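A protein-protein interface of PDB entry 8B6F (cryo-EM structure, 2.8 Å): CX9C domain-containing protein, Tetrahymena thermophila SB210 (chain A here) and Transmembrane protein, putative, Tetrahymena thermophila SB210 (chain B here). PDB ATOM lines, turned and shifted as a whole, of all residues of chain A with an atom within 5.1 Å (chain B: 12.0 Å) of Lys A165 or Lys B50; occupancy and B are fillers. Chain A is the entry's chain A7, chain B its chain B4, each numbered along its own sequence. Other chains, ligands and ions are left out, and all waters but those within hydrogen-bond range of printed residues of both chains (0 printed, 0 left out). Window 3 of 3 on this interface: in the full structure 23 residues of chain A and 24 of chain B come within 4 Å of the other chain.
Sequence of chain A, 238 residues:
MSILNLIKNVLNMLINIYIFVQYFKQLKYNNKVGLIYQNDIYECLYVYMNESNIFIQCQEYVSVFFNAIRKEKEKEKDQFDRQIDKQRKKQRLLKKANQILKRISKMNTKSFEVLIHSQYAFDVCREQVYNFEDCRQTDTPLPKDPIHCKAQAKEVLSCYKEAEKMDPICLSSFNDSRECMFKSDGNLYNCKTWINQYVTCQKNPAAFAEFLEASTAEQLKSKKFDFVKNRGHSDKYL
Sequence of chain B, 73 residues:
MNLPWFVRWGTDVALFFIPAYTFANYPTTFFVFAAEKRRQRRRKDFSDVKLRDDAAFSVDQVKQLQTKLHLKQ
O of Lys A165 sits at hydrogen-bond distance from NE2 of Gln A202, at 3.1 Å.
Lys B50 touches Lys A165 (O to CA, 3.7 Å). Met A166 touches Lys B50 (N to O, 3.6 Å). O of Met A166 touches CA of Leu B51, 3.1 Å away. OD1 of Asp A167 touches CD of Arg B52, 3.3 Å away. Asp A167 touches Ala B55 (OD1 to CA, 3.5 Å).
No residue of chain B comes within 4 Å of Ala A163. Of chain B, only Lys B50 comes within 4 Å of Glu A164. Lys A165 touches just these residues of chain B: Lys B50 (3.7 Å) and Arg B52 (2.9 Å). Of the printed residues of chain B, Gln A202 touches Arg B52 (3.3 Å). Asp B45 touches none of the printed residues of chain A. Of the printed residues of chain A, Lys B50 touches Glu A164, Lys A165 and Met A166. Of the printed residues of chain A, Leu B51 touches Met A166 (3.1 Å). Of the printed residues of chain A, Arg B52 touches Lys A165, Met A166, Asp A167 and Gln A202. Of the printed residues of chain A, Ala B55 touches Asp A167 (3.5 Å). Printed residues of chain A within 4 Å of Ala B56: Asp A167 (3.1 Å). The nearest residue of chain B that does not touch Lys A165 is Leu B51 (4.1 Å). The nearest printed residue of chain A that does not touch Leu B51 is Lys A165 (4.1 Å).
NZ of Lys B50 is in salt-bridge range of OE1 of Glu A164. NE of Arg B52 lies within hydrogen-bond range of O of Lys A165 (2.9 Å). The backbone carbonyl oxygen of Met A166 sits at hydrogen-bond distance from the backbone NH of Arg B52 (3.1 Å). The guanidinium group of Arg B52 sits close to the side-chain amide nitrogen of Gln A202, 3.3 Å away. The side-chain carboxylate (OD2) of Asp A167 lies within hydrogen-bond range of the backbone NH (N) of Ala B56 (3.1 Å).
Of the 9 printed residues of chain A, 5 touch a printed residue of chain B. Printed residues of chain A that touch a printed residue of chain B: Glu A164, Lys A165, Met A166, Asp A167 and Gln A202. Among the printed residues, Asp or Glu carboxylates within 4 Å of a Lys or Arg side-chain nitrogen of the other chain: Glu A164 with Lys B50 (3.2 Å).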
ATOM      1  N   MET A 107      27.660  39.156  31.363  1.00  0.00           N
ATOM      2  CA  MET A 107      27.476  37.878  30.697  1.00  0.00           C
ATOM      3  C   MET A 107      28.100  37.817  29.315  1.00  0.00           C
ATOM      4  O   MET A 107      28.331  36.714  28.810  1.00  0.00           O
ATOM      5  CB  MET A 107      25.983  37.555  30.554  1.00  0.00           C
ATOM      6  CG  MET A 107      25.232  37.448  31.861  1.00  0.00           C
ATOM      7  SD  MET A 107      25.918  36.217  32.981  1.00  0.00           S
ATOM      8  CE  MET A 107      25.970  34.769  31.931  1.00  0.00           C
ATOM      9  N   LYS A 161      25.133  31.321  34.812  1.00  0.00           N
ATOM     10  CA  LYS A 161      26.273  30.878  34.016  1.00  0.00           C
ATOM     11  C   LYS A 161      26.281  29.362  33.885  1.00  0.00           C
ATOM     12  O   LYS A 161      26.499  28.825  32.794  1.00  0.00           O
ATOM     13  CB  LYS A 161      27.578  31.353  34.654  1.00  0.00           C
ATOM     14  CG  LYS A 161      28.103  32.672  34.127  1.00  0.00           C
ATOM     15  CD  LYS A 161      27.600  33.849  34.942  1.00  0.00           C
ATOM     16  CE  LYS A 161      28.410  35.099  34.646  1.00  0.00           C
ATOM     17  NZ  LYS A 161      27.784  36.302  35.254  1.00  0.00           N
ATOM     18  N   GLU A 162      26.046  28.656  34.991  1.00  0.00           N
ATOM     19  CA  GLU A 162      26.004  27.199  34.943  1.00  0.00           C
ATOM     20  C   GLU A 162      24.892  26.712  34.022  1.00  0.00           C
ATOM     21  O   GLU A 162      25.075  25.751  33.268  1.00  0.00           O
ATOM     22  CB  GLU A 162      25.817  26.638  36.353  1.00  0.00           C
ATOM     23  CG  GLU A 162      26.959  26.972  37.306  1.00  0.00           C
ATOM     24  CD  GLU A 162      26.645  26.605  38.742  1.00  0.00           C
ATOM     25  OE1 GLU A 162      25.633  25.909  38.972  1.00  0.00           O
ATOM     26  OE2 GLU A 162      27.404  27.019  39.645  1.00  0.00           O
ATOM     27  N   ALA A 163      23.728  27.363  34.073  1.00  0.00           N
ATOM     28  CA  ALA A 163      22.572  26.892  33.318  1.00  0.00           C
ATOM     29  C   ALA A 163      22.663  27.215  31.833  1.00  0.00           C
ATOM     30  O   ALA A 163      22.076  26.497  31.016  1.00  0.00           O
ATOM     31  CB  ALA A 163      21.292  27.496  33.894  1.00  0.00           C
ATOM     32  N   GLU A 164      23.378  28.278  31.458  1.00  0.00           N
ATOM     33  CA  GLU A 164      23.392  28.701  30.062  1.00  0.00           C
ATOM     34  C   GLU A 164      23.908  27.618  29.124  1.00  0.00           C
ATOM     35  O   GLU A 164      23.602  27.656  27.927  1.00  0.00           O
ATOM     36  CB  GLU A 164      24.239  29.964  29.897  1.00  0.00           C
ATOM     37  CG  GLU A 164      23.447  31.254  30.023  1.00  0.00           C
ATOM     38  CD  GLU A 164      24.212  32.460  29.514  1.00  0.00           C
ATOM     39  OE1 GLU A 164      25.459  32.413  29.504  1.00  0.00           O
ATOM     40  OE2 GLU A 164      23.565  33.452  29.118  1.00  0.00           O
ATOM     41  N   LYS A 165      24.685  26.664  29.629  1.00  0.00           N
ATOM     42  CA  LYS A 165      25.181  25.589  28.780  1.00  0.00           C
ATOM     43  C   LYS A 165      24.022  24.744  28.267  1.00  0.00           C
ATOM     44  O   LYS A 165      23.028  24.533  28.966  1.00  0.00           O
ATOM     45  CB  LYS A 165      26.171  24.720  29.554  1.00  0.00           C
ATOM     46  CG  LYS A 165      27.376  25.485  30.085  1.00  0.00           C
ATOM     47  CD  LYS A 165      28.285  24.583  30.907  1.00  0.00           C
ATOM     48  CE  LYS A 165      29.465  25.360  31.470  1.00  0.00           C
ATOM     49  NZ  LYS A 165      30.371  24.493  32.276  1.00  0.00           N
ATOM     50  N   MET A 166      24.152  24.260  27.033  1.00  0.00           N
ATOM     51  CA  MET A 166      23.105  23.479  26.393  1.00  0.00           C
ATOM     52  C   MET A 166      23.734  22.337  25.609  1.00  0.00           C
ATOM     53  O   MET A 166      24.903  22.390  25.226  1.00  0.00           O
ATOM     54  CB  MET A 166      22.253  24.347  25.455  1.00  0.00           C
ATOM     55  CG  MET A 166      22.973  24.757  24.178  1.00  0.00           C
ATOM     56  SD  MET A 166      22.067  25.992  23.231  1.00  0.00           S
ATOM     57  CE  MET A 166      22.325  27.444  24.245  1.00  0.00           C
ATOM     58  N   ASP A 167      22.941  21.295  25.378  1.00  0.00           N
ATOM     59  CA  ASP A 167      23.394  20.201  24.537  1.00  0.00           C
ATOM     60  C   ASP A 167      23.383  20.627  23.070  1.00  0.00           C
ATOM     61  O   ASP A 167      22.590  21.482  22.670  1.00  0.00           O
ATOM     62  CB  ASP A 167      22.506  18.973  24.719  1.00  0.00           C
ATOM     63  CG  ASP A 167      22.725  18.289  26.051  1.00  0.00           C
ATOM     64  OD1 ASP A 167      23.457  18.844  26.894  1.00  0.00           O
ATOM     65  OD2 ASP A 167      22.171  17.189  26.251  1.00  0.00           O
ATOM     66  N   GLN A 202      16.159  21.336  26.495  1.00  0.00           N
ATOM     67  CA  GLN A 202      17.091  21.472  27.610  1.00  0.00           C
ATOM     68  C   GLN A 202      16.751  20.506  28.737  1.00  0.00           C
ATOM     69  O   GLN A 202      17.644  19.880  29.317  1.00  0.00           O
ATOM     70  CB  GLN A 202      17.080  22.910  28.124  1.00  0.00           C
ATOM     71  CG  GLN A 202      17.841  23.889  27.254  1.00  0.00           C
ATOM     72  CD  GLN A 202      19.336  23.660  27.300  1.00  0.00           C
ATOM     73  OE1 GLN A 202      19.853  22.736  26.675  1.00  0.00           O
ATOM     74  NE2 GLN A 202      20.039  24.497  28.051  1.00  0.00           N
ATOM     75  N   ARG B  43      22.365  32.645  12.053  1.00  0.00           N
ATOM     76  CA  ARG B  43      22.215  31.376  12.751  1.00  0.00           C
ATOM     77  C   ARG B  43      23.538  30.965  13.382  1.00  0.00           C
ATOM     78  O   ARG B  43      24.584  30.977  12.729  1.00  0.00           O
ATOM     79  CB  ARG B  43      21.727  30.304  11.775  1.00  0.00           C
ATOM     80  CG  ARG B  43      21.509  28.941  12.408  1.00  0.00           C
ATOM     81  CD  ARG B  43      20.758  28.015  11.468  1.00  0.00           C
ATOM     82  NE  ARG B  43      19.382  28.451  11.264  1.00  0.00           N
ATOM     83  CZ  ARG B  43      18.346  28.055  11.993  1.00  0.00           C
ATOM     84  NH1 ARG B  43      18.487  27.195  12.988  1.00  0.00           N
ATOM     85  NH2 ARG B  43      17.137  28.534  11.715  1.00  0.00           N
ATOM     86  N   LYS B  44      23.485  30.601  14.662  1.00  0.00           N
ATOM     87  CA  LYS B  44      24.689  30.326  15.428  1.00  0.00           C
ATOM     88  C   LYS B  44      25.210  28.920  15.140  1.00  0.00           C
ATOM     89  O   LYS B  44      24.579  28.118  14.445  1.00  0.00           O
ATOM     90  CB  LYS B  44      24.424  30.496  16.924  1.00  0.00           C
ATOM     91  CG  LYS B  44      24.779  31.872  17.462  1.00  0.00           C
ATOM     92  CD  LYS B  44      24.585  31.935  18.968  1.00  0.00           C
ATOM     93  CE  LYS B  44      24.974  33.294  19.527  1.00  0.00           C
ATOM     94  NZ  LYS B  44      26.420  33.589  19.341  1.00  0.00           N
ATOM     95  N   ASP B  45      26.382  28.627  15.696  1.00  0.00           N
ATOM     96  CA  ASP B  45      27.077  27.367  15.489  1.00  0.00           C
ATOM     97  C   ASP B  45      27.474  26.779  16.836  1.00  0.00           C
ATOM     98  O   ASP B  45      27.420  27.446  17.872  1.00  0.00           O
ATOM     99  CB  ASP B  45      28.315  27.562  14.602  1.00  0.00           C
ATOM    100  CG  ASP B  45      28.902  26.250  14.121  1.00  0.00           C
ATOM    101  OD1 ASP B  45      28.336  25.188  14.453  1.00  0.00           O
ATOM    102  OD2 ASP B  45      29.931  26.281  13.414  1.00  0.00           O
ATOM    103  N   PHE B  46      27.881  25.508  16.810  1.00  0.00           N
ATOM    104  CA  PHE B  46      28.314  24.839  18.033  1.00  0.00           C
ATOM    105  C   PHE B  46      29.519  25.538  18.649  1.00  0.00           C
ATOM    106  O   PHE B  46      29.580  25.728  19.869  1.00  0.00           O
ATOM    107  CB  PHE B  46      28.638  23.374  17.742  1.00  0.00           C
ATOM    108  CG  PHE B  46      27.488  22.604  17.163  1.00  0.00           C
ATOM    109  CD1 PHE B  46      26.502  22.088  17.987  1.00  0.00           C
ATOM    110  CD2 PHE B  46      27.399  22.384  15.800  1.00  0.00           C
ATOM    111  CE1 PHE B  46      25.442  21.377  17.460  1.00  0.00           C
ATOM    112  CE2 PHE B  46      26.342  21.673  15.267  1.00  0.00           C
ATOM    113  CZ  PHE B  46      25.361  21.168  16.099  1.00  0.00           C
ATOM    114  N   SER B  47      30.490  25.926  17.823  1.00  0.00           N
ATOM    115  CA  SER B  47      31.656  26.635  18.338  1.00  0.00           C
ATOM    116  C   SER B  47      31.259  27.975  18.944  1.00  0.00           C
ATOM    117  O   SER B  47      31.779  28.367  19.995  1.00  0.00           O
ATOM    118  CB  SER B  47      32.686  26.832  17.224  1.00  0.00           C
ATOM    119  OG  SER B  47      32.148  27.596  16.159  1.00  0.00           O
ATOM    120  N   ASP B  48      30.338  28.694  18.298  1.00  0.00           N
ATOM    121  CA  ASP B  48      29.896  29.978  18.835  1.00  0.00           C
ATOM    122  C   ASP B  48      29.228  29.809  20.194  1.00  0.00           C
ATOM    123  O   ASP B  48      29.471  30.597  21.114  1.00  0.00           O
ATOM    124  CB  ASP B  48      28.939  30.653  17.852  1.00  0.00           C
ATOM    125  CG  ASP B  48      29.589  30.947  16.514  1.00  0.00           C
ATOM    126  OD1 ASP B  48      30.805  30.704  16.376  1.00  0.00           O
ATOM    127  OD2 ASP B  48      28.882  31.416  15.597  1.00  0.00           O
ATOM    128  N   VAL B  49      28.381  28.791  20.341  1.00  0.00           N
ATOM    129  CA  VAL B  49      27.729  28.541  21.621  1.00  0.00           C
ATOM    130  C   VAL B  49      28.645  27.706  22.510  1.00  0.00           C
ATOM    131  O   VAL B  49      29.616  27.098  22.056  1.00  0.00           O
ATOM    132  CB  VAL B  49      26.363  27.854  21.428  1.00  0.00           C
ATOM    133  CG1 VAL B  49      25.472  28.679  20.510  1.00  0.00           C
ATOM    134  CG2 VAL B  49      26.538  26.442  20.883  1.00  0.00           C
ATOM    135  N   LYS B  50      28.329  27.685  23.801  1.00  0.00           N
ATOM    136  CA  LYS B  50      29.035  26.865  24.776  1.00  0.00           C
ATOM    137  C   LYS B  50      28.137  25.709  25.190  1.00  0.00           C
ATOM    138  O   LYS B  50      26.969  25.917  25.533  1.00  0.00           O
ATOM    139  CB  LYS B  50      29.452  27.692  25.995  1.00  0.00           C
ATOM    140  CG  LYS B  50      28.310  28.413  26.690  1.00  0.00           C
ATOM    141  CD  LYS B  50      28.823  29.229  27.868  1.00  0.00           C
ATOM    142  CE  LYS B  50      27.692  29.974  28.558  1.00  0.00           C
ATOM    143  NZ  LYS B  50      28.178  30.769  29.720  1.00  0.00           N
ATOM    144  N   LEU B  51      28.683  24.498  25.158  1.00  0.00           N
ATOM    145  CA  LEU B  51      27.911  23.278  25.328  1.00  0.00           C
ATOM    146  C   LEU B  51      28.182  22.648  26.688  1.00  0.00           C
ATOM    147  O   LEU B  51      29.219  22.881  27.315  1.00  0.00           O
ATOM    148  CB  LEU B  51      28.238  22.272  24.218  1.00  0.00           C
ATOM    149  CG  LEU B  51      28.140  22.806  22.787  1.00  0.00           C
ATOM    150  CD1 LEU B  51      28.580  21.745  21.791  1.00  0.00           C
ATOM    151  CD2 LEU B  51      26.728  23.278  22.480  1.00  0.00           C
ATOM    152  N   ARG B  52      27.224  21.841  27.138  1.00  0.00           N
ATOM    153  CA  ARG B  52      27.375  21.107  28.384  1.00  0.00           C
ATOM    154  C   ARG B  52      28.395  19.987  28.228  1.00  0.00           C
ATOM    155  O   ARG B  52      28.610  19.458  27.136  1.00  0.00           O
ATOM    156  CB  ARG B  52      26.036  20.515  28.824  1.00  0.00           C
ATOM    157  CG  ARG B  52      24.968  21.542  29.145  1.00  0.00           C
ATOM    158  CD  ARG B  52      23.659  20.863  29.515  1.00  0.00           C
ATOM    159  NE  ARG B  52      22.636  21.821  29.911  1.00  0.00           N
ATOM    160  CZ  ARG B  52      21.393  21.498  30.241  1.00  0.00           C
ATOM    161  NH1 ARG B  52      20.978  20.241  30.227  1.00  0.00           N
ATOM    162  NH2 ARG B  52      20.546  22.459  30.595  1.00  0.00           N
ATOM    163  N   ASP B  53      29.029  19.627  29.346  1.00  0.00           N
ATOM    164  CA  ASP B  53      29.975  18.517  29.331  1.00  0.00           C
ATOM    165  C   ASP B  53      29.255  17.180  29.200  1.00  0.00           C
ATOM    166  O   ASP B  53      29.666  16.320  28.413  1.00  0.00           O
ATOM    167  CB  ASP B  53      30.829  18.540  30.597  1.00  0.00           C
ATOM    168  CG  ASP B  53      31.600  19.834  30.755  1.00  0.00           C
ATOM    169  OD1 ASP B  53      32.013  20.409  29.725  1.00  0.00           O
ATOM    170  OD2 ASP B  53      31.790  20.279  31.906  1.00  0.00           O
ATOM    171  N   ASP B  54      28.179  16.990  29.961  1.00  0.00           N
ATOM    172  CA  ASP B  54      27.421  15.739  29.935  1.00  0.00           C
ATOM    173  C   ASP B  54      26.287  15.825  28.912  1.00  0.00           C
ATOM    174  O   ASP B  54      25.104  15.703  29.227  1.00  0.00           O
ATOM    175  CB  ASP B  54      26.891  15.413  31.327  1.00  0.00           C
ATOM    176  CG  ASP B  54      25.969  16.489  31.869  1.00  0.00           C
ATOM    177  OD1 ASP B  54      25.788  17.521  31.187  1.00  0.00           O
ATOM    178  OD2 ASP B  54      25.421  16.301  32.975  1.00  0.00           O
ATOM    179  N   ALA B  55      26.676  16.041  27.660  1.00  0.00           N
ATOM    180  CA  ALA B  55      25.714  16.132  26.571  1.00  0.00           C
ATOM    181  C   ALA B  55      25.220  14.739  26.200  1.00  0.00           C
ATOM    182  O   ALA B  55      26.018  13.817  26.009  1.00  0.00           O
ATOM    183  CB  ALA B  55      26.342  16.813  25.358  1.00  0.00           C
ATOM    184  N   ALA B  56      23.898  14.591  26.094  1.00  0.00           N
ATOM    185  CA  ALA B  56      23.331  13.296  25.738  1.00  0.00           C
ATOM    186  C   ALA B  56      23.805  12.850  24.362  1.00  0.00           C
ATOM    187  O   ALA B  56      24.129  11.674  24.158  1.00  0.00           O
ATOM    188  CB  ALA B  56      21.806  13.361  25.784  1.00  0.00           C
ATOM    189  N   PHE B  57      23.851  13.773  23.407  1.00  0.00           N
ATOM    190  CA  PHE B  57      24.321  13.502  22.058  1.00  0.00           C
ATOM    191  C   PHE B  57      25.496  14.415  21.742  1.00  0.00           C
ATOM    192  O   PHE B  57      25.458  15.613  22.035  1.00  0.00           O
ATOM    193  CB  PHE B  57      23.203  13.709  21.029  1.00  0.00           C
ATOM    194  CG  PHE B  57      22.088  12.712  21.142  1.00  0.00           C
ATOM    195  CD1 PHE B  57      21.122  12.840  22.128  1.00  0.00           C
ATOM    196  CD2 PHE B  57      22.000  11.649  20.258  1.00  0.00           C
ATOM    197  CE1 PHE B  57      20.093  11.924  22.233  1.00  0.00           C
ATOM    198  CE2 PHE B  57      20.974  10.729  20.358  1.00  0.00           C
ATOM    199  CZ  PHE B  57      20.018  10.867  21.347  1.00  0.00           C
ATOM    200  N   SER B  58      26.540  13.845  21.149  1.00  0.00           N
ATOM    201  CA  SER B  58      27.691  14.635  20.749  1.00  0.00           C
ATOM    202  C   SER B  58      27.348  15.483  19.527  1.00  0.00           C
ATOM    203  O   SER B  58      26.292  15.335  18.906  1.00  0.00           O
ATOM    204  CB  SER B  58      28.885  13.729  20.451  1.00  0.00           C
ATOM    205  OG  SER B  58      28.602  12.851  19.377  1.00  0.00           O
ATOM    206  N   VAL B  59      28.263  16.389  19.180  1.00  0.00           N
ATOM    207  CA  VAL B  59      28.039  17.262  18.030  1.00  0.00           C
ATOM    208  C   VAL B  59      27.929  16.439  16.754  1.00  0.00           C
ATOM    209  O   VAL B  59      27.059  16.688  15.910  1.00  0.00           O
ATOM    210  CB  VAL B  59      29.159  18.316  17.933  1.00  0.00           C
ATOM    211  CG1 VAL B  59      28.982  19.177  16.690  1.00  0.00           C
ATOM    212  CG2 VAL B  59      29.179  19.182  19.181  1.00  0.00           C
